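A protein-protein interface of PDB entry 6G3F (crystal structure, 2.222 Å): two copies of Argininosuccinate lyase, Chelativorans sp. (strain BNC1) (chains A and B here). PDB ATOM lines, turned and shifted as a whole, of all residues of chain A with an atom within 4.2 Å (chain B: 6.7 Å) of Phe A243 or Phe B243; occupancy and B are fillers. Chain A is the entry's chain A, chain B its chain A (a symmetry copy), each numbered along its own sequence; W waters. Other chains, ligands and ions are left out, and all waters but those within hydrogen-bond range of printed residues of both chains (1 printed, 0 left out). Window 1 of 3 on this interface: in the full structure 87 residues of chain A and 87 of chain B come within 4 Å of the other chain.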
ATOM      1  N   ALA A 239      20.889 -31.277  12.599  1.00  0.00           N
ATOM      2  CA  ALA A 239      21.998 -30.672  11.874  1.00  0.00           C
ATOM      3  C   ALA A 239      23.205 -31.599  11.844  1.00  0.00           C
ATOM      4  O   ALA A 239      23.859 -31.746  10.804  1.00  0.00           O
ATOM      5  CB  ALA A 239      22.369 -29.336  12.513  1.00  0.00           C
ATOM      6  N   GLU A 240      23.515 -32.234  12.980  1.00  0.00           N
ATOM      7  CA  GLU A 240      24.692 -33.094  13.053  1.00  0.00           C
ATOM      8  C   GLU A 240      24.519 -34.331  12.186  1.00  0.00           C
ATOM      9  O   GLU A 240      25.464 -34.760  11.512  1.00  0.00           O
ATOM     10  CB  GLU A 240      24.971 -33.489  14.505  1.00  0.00           C
ATOM     11  CG  GLU A 240      26.237 -34.321  14.676  1.00  0.00           C
ATOM     12  CD  GLU A 240      26.511 -34.705  16.117  1.00  0.00           C
ATOM     13  OE1 GLU A 240      25.871 -34.132  17.026  1.00  0.00           O
ATOM     14  OE2 GLU A 240      27.369 -35.587  16.335  1.00  0.00           O
ATOM     15  N   HIS A 241      23.323 -34.919  12.190  1.00  0.00           N
ATOM     16  CA  HIS A 241      23.055 -36.042  11.301  1.00  0.00           C
ATOM     17  C   HIS A 241      23.307 -35.642   9.854  1.00  0.00           C
ATOM     18  O   HIS A 241      23.960 -36.369   9.097  1.00  0.00           O
ATOM     19  CB  HIS A 241      21.619 -36.524  11.499  1.00  0.00           C
ATOM     20  CG  HIS A 241      21.356 -37.894  10.958  1.00  0.00           C
ATOM     21  ND1 HIS A 241      20.365 -38.710  11.460  1.00  0.00           N
ATOM     22  CD2 HIS A 241      21.947 -38.590   9.958  1.00  0.00           C
ATOM     23  CE1 HIS A 241      20.360 -39.851  10.793  1.00  0.00           C
ATOM     24  NE2 HIS A 241      21.309 -39.803   9.876  1.00  0.00           N
ATOM     25  N   ALA A 242      22.814 -34.467   9.458  1.00  0.00           N
ATOM     26  CA  ALA A 242      23.056 -33.983   8.106  1.00  0.00           C
ATOM     27  C   ALA A 242      24.546 -33.798   7.845  1.00  0.00           C
ATOM     28  O   ALA A 242      25.029 -34.080   6.742  1.00  0.00           O
ATOM     29  CB  ALA A 242      22.303 -32.671   7.875  1.00  0.00           C
ATOM     30  N   PHE A 243      25.297 -33.327   8.845  1.00  0.00           N
ATOM     31  CA  PHE A 243      26.715 -33.072   8.617  1.00  0.00           C
ATOM     32  C   PHE A 243      27.493 -34.366   8.414  1.00  0.00           C
ATOM     33  O   PHE A 243      28.279 -34.483   7.467  1.00  0.00           O
ATOM     34  CB  PHE A 243      27.343 -32.295   9.769  1.00  0.00           C
ATOM     35  CG  PHE A 243      28.838 -32.354   9.740  1.00  0.00           C
ATOM     36  CD1 PHE A 243      29.542 -31.645   8.785  1.00  0.00           C
ATOM     37  CD2 PHE A 243      29.536 -33.170  10.614  1.00  0.00           C
ATOM     38  CE1 PHE A 243      30.915 -31.717   8.722  1.00  0.00           C
ATOM     39  CE2 PHE A 243      30.915 -33.244  10.556  1.00  0.00           C
ATOM     40  CZ  PHE A 243      31.603 -32.520   9.606  1.00  0.00           C
ATOM     41  N   VAL A 244      27.334 -35.330   9.325  1.00  0.00           N
ATOM     42  CA  VAL A 244      28.085 -36.576   9.193  1.00  0.00           C
ATOM     43  C   VAL A 244      27.785 -37.218   7.849  1.00  0.00           C
ATOM     44  O   VAL A 244      28.688 -37.719   7.168  1.00  0.00           O
ATOM     45  CB  VAL A 244      27.782 -37.532  10.364  1.00  0.00           C
ATOM     46  CG1 VAL A 244      28.637 -38.792  10.250  1.00  0.00           C
ATOM     47  CG2 VAL A 244      28.052 -36.852  11.700  1.00  0.00           C
ATOM     48  N   ASN A 245      26.516 -37.199   7.436  1.00  0.00           N
ATOM     49  CA  ASN A 245      26.162 -37.652   6.095  1.00  0.00           C
ATOM     50  C   ASN A 245      26.985 -36.918   5.044  1.00  0.00           C
ATOM     51  O   ASN A 245      27.543 -37.534   4.129  1.00  0.00           O
ATOM     52  CB  ASN A 245      24.666 -37.439   5.847  1.00  0.00           C
ATOM     53  CG  ASN A 245      23.795 -38.476   6.542  1.00  0.00           C
ATOM     54  OD1 ASN A 245      24.280 -39.301   7.317  1.00  0.00           O
ATOM     55  ND2 ASN A 245      22.496 -38.432   6.264  1.00  0.00           N
ATOM     56  N   ALA A 246      27.083 -35.592   5.171  1.00  0.00           N
ATOM     57  CA  ALA A 246      27.776 -34.792   4.166  1.00  0.00           C
ATOM     58  C   ALA A 246      29.269 -35.105   4.133  1.00  0.00           C
ATOM     59  O   ALA A 246      29.845 -35.300   3.056  1.00  0.00           O
ATOM     60  CB  ALA A 246      27.545 -33.305   4.432  1.00  0.00           C
ATOM     61  N   VAL A 247      29.920 -35.151   5.298  1.00  0.00           N
ATOM     62  CA  VAL A 247      31.367 -35.354   5.311  1.00  0.00           C
ATOM     63  C   VAL A 247      31.708 -36.792   4.941  1.00  0.00           C
ATOM     64  O   VAL A 247      32.686 -37.044   4.226  1.00  0.00           O
ATOM     65  CB  VAL A 247      31.966 -34.951   6.672  1.00  0.00           C
ATOM     66  CG1 VAL A 247      31.574 -35.934   7.772  1.00  0.00           C
ATOM     67  CG2 VAL A 247      33.482 -34.830   6.565  1.00  0.00           C
ATOM     68  N   LEU A 306      22.035 -30.036   5.056  1.00  0.00           N
ATOM     69  CA  LEU A 306      22.906 -29.446   6.064  1.00  0.00           C
ATOM     70  C   LEU A 306      22.768 -27.927   6.089  1.00  0.00           C
ATOM     71  O   LEU A 306      22.641 -27.319   7.158  1.00  0.00           O
ATOM     72  CB  LEU A 306      24.353 -29.860   5.787  1.00  0.00           C
ATOM     73  CG  LEU A 306      25.457 -29.211   6.624  1.00  0.00           C
ATOM     74  CD1 LEU A 306      25.298 -29.550   8.098  1.00  0.00           C
ATOM     75  CD2 LEU A 306      26.814 -29.657   6.107  1.00  0.00           C
ATOM     76  N   ARG B 185      30.571 -32.438  21.519  1.00  0.00           N
ATOM     77  CA  ARG B 185      30.990 -32.386  20.120  1.00  0.00           C
ATOM     78  C   ARG B 185      32.434 -31.925  20.001  1.00  0.00           C
ATOM     79  O   ARG B 185      33.234 -32.521  19.272  1.00  0.00           O
ATOM     80  CB  ARG B 185      30.076 -31.450  19.325  1.00  0.00           C
ATOM     81  CG  ARG B 185      28.666 -31.961  19.152  1.00  0.00           C
ATOM     82  CD  ARG B 185      27.860 -31.099  18.190  1.00  0.00           C
ATOM     83  NE  ARG B 185      26.532 -31.668  17.990  1.00  0.00           N
ATOM     84  CZ  ARG B 185      25.446 -31.325  18.676  1.00  0.00           C
ATOM     85  NH1 ARG B 185      25.498 -30.386  19.611  1.00  0.00           N
ATOM     86  NH2 ARG B 185      24.293 -31.928  18.417  1.00  0.00           N
ATOM     87  N   TYR B 186      32.783 -30.854  20.716  1.00  0.00           N
ATOM     88  CA  TYR B 186      34.131 -30.305  20.629  1.00  0.00           C
ATOM     89  C   TYR B 186      35.163 -31.284  21.178  1.00  0.00           C
ATOM     90  O   TYR B 186      36.220 -31.487  20.568  1.00  0.00           O
ATOM     91  CB  TYR B 186      34.193 -28.972  21.378  1.00  0.00           C
ATOM     92  CG  TYR B 186      33.744 -27.766  20.572  1.00  0.00           C
ATOM     93  CD1 TYR B 186      34.279 -27.503  19.316  1.00  0.00           C
ATOM     94  CD2 TYR B 186      32.791 -26.886  21.069  1.00  0.00           C
ATOM     95  CE1 TYR B 186      33.879 -26.399  18.579  1.00  0.00           C
ATOM     96  CE2 TYR B 186      32.382 -25.777  20.335  1.00  0.00           C
ATOM     97  CZ  TYR B 186      32.934 -25.540  19.092  1.00  0.00           C
ATOM     98  OH  TYR B 186      32.542 -24.447  18.351  1.00  0.00           O
ATOM     99  N   ASP B 236      38.795 -34.401   7.121  1.00  0.00           N
ATOM    100  CA  ASP B 236      37.463 -34.406   7.713  1.00  0.00           C
ATOM    101  C   ASP B 236      37.437 -33.672   9.046  1.00  0.00           C
ATOM    102  O   ASP B 236      36.409 -33.094   9.413  1.00  0.00           O
ATOM    103  CB  ASP B 236      36.985 -35.847   7.891  1.00  0.00           C
ATOM    104  CG  ASP B 236      36.705 -36.537   6.567  1.00  0.00           C
ATOM    105  OD1 ASP B 236      36.960 -35.924   5.508  1.00  0.00           O
ATOM    106  OD2 ASP B 236      36.235 -37.694   6.581  1.00  0.00           O
ATOM    107  N   VAL B 238      38.884 -30.969   9.657  1.00  0.00           N
ATOM    108  CA  VAL B 238      38.718 -29.550   9.346  1.00  0.00           C
ATOM    109  C   VAL B 238      37.249 -29.240   9.086  1.00  0.00           C
ATOM    110  O   VAL B 238      36.697 -28.265   9.608  1.00  0.00           O
ATOM    111  CB  VAL B 238      39.589 -29.157   8.138  1.00  0.00           C
ATOM    112  CG1 VAL B 238      39.561 -27.649   7.932  1.00  0.00           C
ATOM    113  CG2 VAL B 238      41.024 -29.650   8.308  1.00  0.00           C
ATOM    114  N   ALA B 239      36.598 -30.064   8.265  1.00  0.00           N
ATOM    115  CA  ALA B 239      35.167 -29.910   8.037  1.00  0.00           C
ATOM    116  C   ALA B 239      34.391 -29.999   9.342  1.00  0.00           C
ATOM    117  O   ALA B 239      33.466 -29.212   9.579  1.00  0.00           O
ATOM    118  CB  ALA B 239      34.681 -30.974   7.055  1.00  0.00           C
ATOM    119  N   GLU B 240      34.755 -30.954  10.206  1.00  0.00           N
ATOM    120  CA  GLU B 240      34.024 -31.146  11.454  1.00  0.00           C
ATOM    121  C   GLU B 240      34.220 -29.963  12.388  1.00  0.00           C
ATOM    122  O   GLU B 240      33.270 -29.521  13.047  1.00  0.00           O
ATOM    123  CB  GLU B 240      34.464 -32.445  12.132  1.00  0.00           C
ATOM    124  CG  GLU B 240      33.685 -32.762  13.404  1.00  0.00           C
ATOM    125  CD  GLU B 240      34.122 -34.053  14.068  1.00  0.00           C
ATOM    126  OE1 GLU B 240      34.853 -34.842  13.430  1.00  0.00           O
ATOM    127  OE2 GLU B 240      33.731 -34.273  15.234  1.00  0.00           O
ATOM    128  N   HIS B 241      35.442 -29.437  12.463  1.00  0.00           N
ATOM    129  CA  HIS B 241      35.677 -28.236  13.254  1.00  0.00           C
ATOM    130  C   HIS B 241      34.776 -27.105  12.777  1.00  0.00           C
ATOM    131  O   HIS B 241      34.140 -26.416  13.583  1.00  0.00           O
ATOM    132  CB  HIS B 241      37.151 -27.842  13.166  1.00  0.00           C
ATOM    133  CG  HIS B 241      37.592 -26.892  14.235  1.00  0.00           C
ATOM    134  ND1 HIS B 241      38.898 -26.820  14.668  1.00  0.00           N
ATOM    135  CD2 HIS B 241      36.905 -25.971  14.952  1.00  0.00           C
ATOM    136  CE1 HIS B 241      38.996 -25.897  15.609  1.00  0.00           C
ATOM    137  NE2 HIS B 241      37.802 -25.367  15.799  1.00  0.00           N
ATOM    138  N   ALA B 242      34.691 -26.916  11.459  1.00  0.00           N
ATOM    139  CA  ALA B 242      33.809 -25.892  10.915  1.00  0.00           C
ATOM    140  C   ALA B 242      32.356 -26.163  11.285  1.00  0.00           C
ATOM    141  O   ALA B 242      31.597 -25.229  11.569  1.00  0.00           O
ATOM    142  CB  ALA B 242      33.972 -25.811   9.397  1.00  0.00           C
ATOM    143  N   PHE B 243      31.945 -27.435  11.291  1.00  0.00           N
ATOM    144  CA  PHE B 243      30.545 -27.733  11.573  1.00  0.00           C
ATOM    145  C   PHE B 243      30.188 -27.432  13.023  1.00  0.00           C
ATOM    146  O   PHE B 243      29.174 -26.778  13.297  1.00  0.00           O
ATOM    147  CB  PHE B 243      30.205 -29.189  11.275  1.00  0.00           C
ATOM    148  CG  PHE B 243      28.912 -29.606  11.902  1.00  0.00           C
ATOM    149  CD1 PHE B 243      27.712 -29.147  11.390  1.00  0.00           C
ATOM    150  CD2 PHE B 243      28.893 -30.393  13.041  1.00  0.00           C
ATOM    151  CE1 PHE B 243      26.516 -29.493  11.977  1.00  0.00           C
ATOM    152  CE2 PHE B 243      27.694 -30.743  13.634  1.00  0.00           C
ATOM    153  CZ  PHE B 243      26.506 -30.288  13.101  1.00  0.00           C
ATOM    154  N   VAL B 244      30.975 -27.947  13.972  1.00  0.00           N
ATOM    155  CA  VAL B 244      30.653 -27.715  15.378  1.00  0.00           C
ATOM    156  C   VAL B 244      30.592 -26.222  15.653  1.00  0.00           C
ATOM    157  O   VAL B 244      29.698 -25.741  16.359  1.00  0.00           O
ATOM    158  CB  VAL B 244      31.662 -28.426  16.301  1.00  0.00           C
ATOM    159  CG1 VAL B 244      31.263 -28.238  17.763  1.00  0.00           C
ATOM    160  CG2 VAL B 244      31.735 -29.913  15.980  1.00  0.00           C
ATOM    161  N   ASN B 245      31.530 -25.460  15.085  1.00  0.00           N
ATOM    162  CA  ASN B 245      31.459 -24.005  15.167  1.00  0.00           C
ATOM    163  C   ASN B 245      30.112 -23.503  14.664  1.00  0.00           C
ATOM    164  O   ASN B 245      29.463 -22.672  15.308  1.00  0.00           O
ATOM    165  CB  ASN B 245      32.599 -23.378  14.359  1.00  0.00           C
ATOM    166  CG  ASN B 245      33.943 -23.459  15.068  1.00  0.00           C
ATOM    167  OD1 ASN B 245      34.075 -24.087  16.119  1.00  0.00           O
ATOM    168  ND2 ASN B 245      34.952 -22.818  14.486  1.00  0.00           N
ATOM    169  N   ALA B 246      29.669 -24.014  13.512  1.00  0.00           N
ATOM    170  CA  ALA B 246      28.431 -23.532  12.906  1.00  0.00           C
ATOM    171  C   ALA B 246      27.217 -23.874  13.763  1.00  0.00           C
ATOM    172  O   ALA B 246      26.360 -23.016  14.007  1.00  0.00           O
ATOM    173  CB  ALA B 246      28.278 -24.112  11.500  1.00  0.00           C
ATOM    174  N   VAL B 247      27.114 -25.123  14.225  1.00  0.00           N
ATOM    175  CA  VAL B 247      25.924 -25.523  14.971  1.00  0.00           C
ATOM    176  C   VAL B 247      25.926 -24.896  16.359  1.00  0.00           C
ATOM    177  O   VAL B 247      24.877 -24.476  16.862  1.00  0.00           O
ATOM    178  CB  VAL B 247      25.805 -27.058  15.032  1.00  0.00           C
ATOM    179  CG1 VAL B 247      26.872 -27.669  15.935  1.00  0.00           C
ATOM    180  CG2 VAL B 247      24.407 -27.460  15.492  1.00  0.00           C
ATOM    181  N   PHE B 248      27.097 -24.809  16.997  1.00  0.00           N
ATOM    182  CA  PHE B 248      27.184 -24.123  18.284  1.00  0.00           C
ATOM    183  C   PHE B 248      26.737 -22.673  18.156  1.00  0.00           C
ATOM    184  O   PHE B 248      25.949 -22.178  18.970  1.00  0.00           O
ATOM    185  CB  PHE B 248      28.612 -24.189  18.833  1.00  0.00           C
ATOM    186  CG  PHE B 248      28.918 -23.103  19.834  1.00  0.00           C
ATOM    187  CD1 PHE B 248      28.366 -23.137  21.104  1.00  0.00           C
ATOM    188  CD2 PHE B 248      29.748 -22.041  19.499  1.00  0.00           C
ATOM    189  CE1 PHE B 248      28.633 -22.136  22.023  1.00  0.00           C
ATOM    190  CE2 PHE B 248      30.022 -21.038  20.414  1.00  0.00           C
ATOM    191  CZ  PHE B 248      29.462 -21.085  21.676  1.00  0.00           C
ATOM    192  N   LEU B 249      27.237 -21.972  17.138  1.00  0.00           N
ATOM    193  CA  LEU B 249      26.878 -20.572  16.957  1.00  0.00           C
ATOM    194  C   LEU B 249      25.423 -20.393  16.549  1.00  0.00           C
ATOM    195  O   LEU B 249      24.852 -19.328  16.804  1.00  0.00           O
ATOM    196  CB  LEU B 249      27.800 -19.924  15.919  1.00  0.00           C
ATOM    197  CG  LEU B 249      29.208 -19.581  16.414  1.00  0.00           C
ATOM    198  CD1 LEU B 249      30.117 -19.185  15.257  1.00  0.00           C
ATOM    199  CD2 LEU B 249      29.157 -18.465  17.449  1.00  0.00           C
ATOM    200  N   ALA B 302      29.760 -18.188   9.905  1.00  0.00           N
ATOM    201  CA  ALA B 302      30.365 -19.497  10.127  1.00  0.00           C
ATOM    202  C   ALA B 302      29.817 -20.560   9.185  1.00  0.00           C
ATOM    203  O   ALA B 302      30.428 -21.627   9.061  1.00  0.00           O
ATOM    204  CB  ALA B 302      30.159 -19.929  11.578  1.00  0.00           C
ATOM    205  N   LEU B 306      32.306 -23.886   6.484  1.00  0.00           N
ATOM    206  CA  LEU B 306      31.756 -25.234   6.429  1.00  0.00           C
ATOM    207  C   LEU B 306      31.420 -25.632   4.996  1.00  0.00           C
ATOM    208  O   LEU B 306      31.756 -26.734   4.547  1.00  0.00           O
ATOM    209  CB  LEU B 306      30.518 -25.312   7.326  1.00  0.00           C
ATOM    210  CG  LEU B 306      29.682 -26.592   7.282  1.00  0.00           C
ATOM    211  CD1 LEU B 306      30.494 -27.793   7.743  1.00  0.00           C
ATOM    212  CD2 LEU B 306      28.439 -26.416   8.138  1.00  0.00           C
ATOM    213  N   LEU B 310      33.623 -28.402   2.675  1.00  0.00           N
ATOM    214  CA  LEU B 310      32.970 -29.606   2.175  1.00  0.00           C
ATOM    215  C   LEU B 310      32.894 -29.603   0.653  1.00  0.00           C
ATOM    216  O   LEU B 310      33.043 -30.653   0.017  1.00  0.00           O
ATOM    217  CB  LEU B 310      31.572 -29.740   2.781  1.00  0.00           C
ATOM    218  CG  LEU B 310      31.531 -30.259   4.220  1.00  0.00           C
ATOM    219  CD1 LEU B 310      30.146 -30.075   4.814  1.00  0.00           C
ATOM    220  CD2 LEU B 310      31.946 -31.731   4.278  1.00  0.00           C
HETATM  221  O   HOH W   1      34.712 -38.795   4.767  1.00  0.00           O
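Water W1 lies within hydrogen-bond range of the side-chain carboxylate (OD2) of Asp B236 (2.6 Å) and the backbone carbonyl oxygen (O) of Val A247 (2.7 Å).
Among the printed residues, pairs that only touch across the chains: Phe A243 with Glu B240, Glu A240 with Phe B243, Phe A243 with Phe B243, Leu A306 with Leu B310, Val A247 with Asp B236, Ala A239 with Phe B243, Phe A243 with Ala B239 and Val A247 with Leu B310.
Ala A239 touches Phe B243, and with the chains exchanged Phe A243 touches Ala B239. Glu A240 touches Phe B243, and with the chains exchanged Phe A243 touches Glu B240. Phe B243 touches its own counterpart, Phe A243. Of the 9 pairs that touch across the chains among the printed residues, 5 have their exchanged pair printed and touching as well.
Of the 10 printed residues of chain A, 5 touch a printed residue of chain B. Printed residues of chain A that touch a printed residue of chain B: Ala A239, Glu A240, Phe A243, Val A247 and Leu A306. Printed residues of chain B that touch a printed residue of chain A: Arg B185, Asp B236, Ala B239, Glu B240, Phe B243 and Leu B310. Hydrophobic or aromatic side chains of chain B within 4 Å of the printed part of chain A: Phe B243 and Leu B310. Among the printed residues, Asp or Glu carboxylates within 4 Å of a Lys or Arg side-chain nitrogen of the other chain: Glu A240 with Arg B185 (2.7 Å).
The side-chain carboxylate (OE1) of Glu A240 lies within salt-bridge range of the guanidinium group (NE) of Arg B185 (2.7 Å).
Of the printed residues of chain B, Ala A239 touches Phe B243 (3.7 Å). Of chain B, only Ala B239, Glu B240 and Phe B243 come within 4 Å of Phe A243. Of the printed residues of chain B, Val A247 touches Asp B236 and Leu B310. Of the printed residues of chain B, Leu A306 touches Leu B310. Printed residues of chain A within 4 Å of Asp B236: Val A247 (3.6 Å). Printed residues of chain A within 4 Å of Ala B239: Phe A243. Phe B243 touches three residues of chain A. The nearest residue of chain B that does not touch Phe A243 is Leu B306 (4.1 Å).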
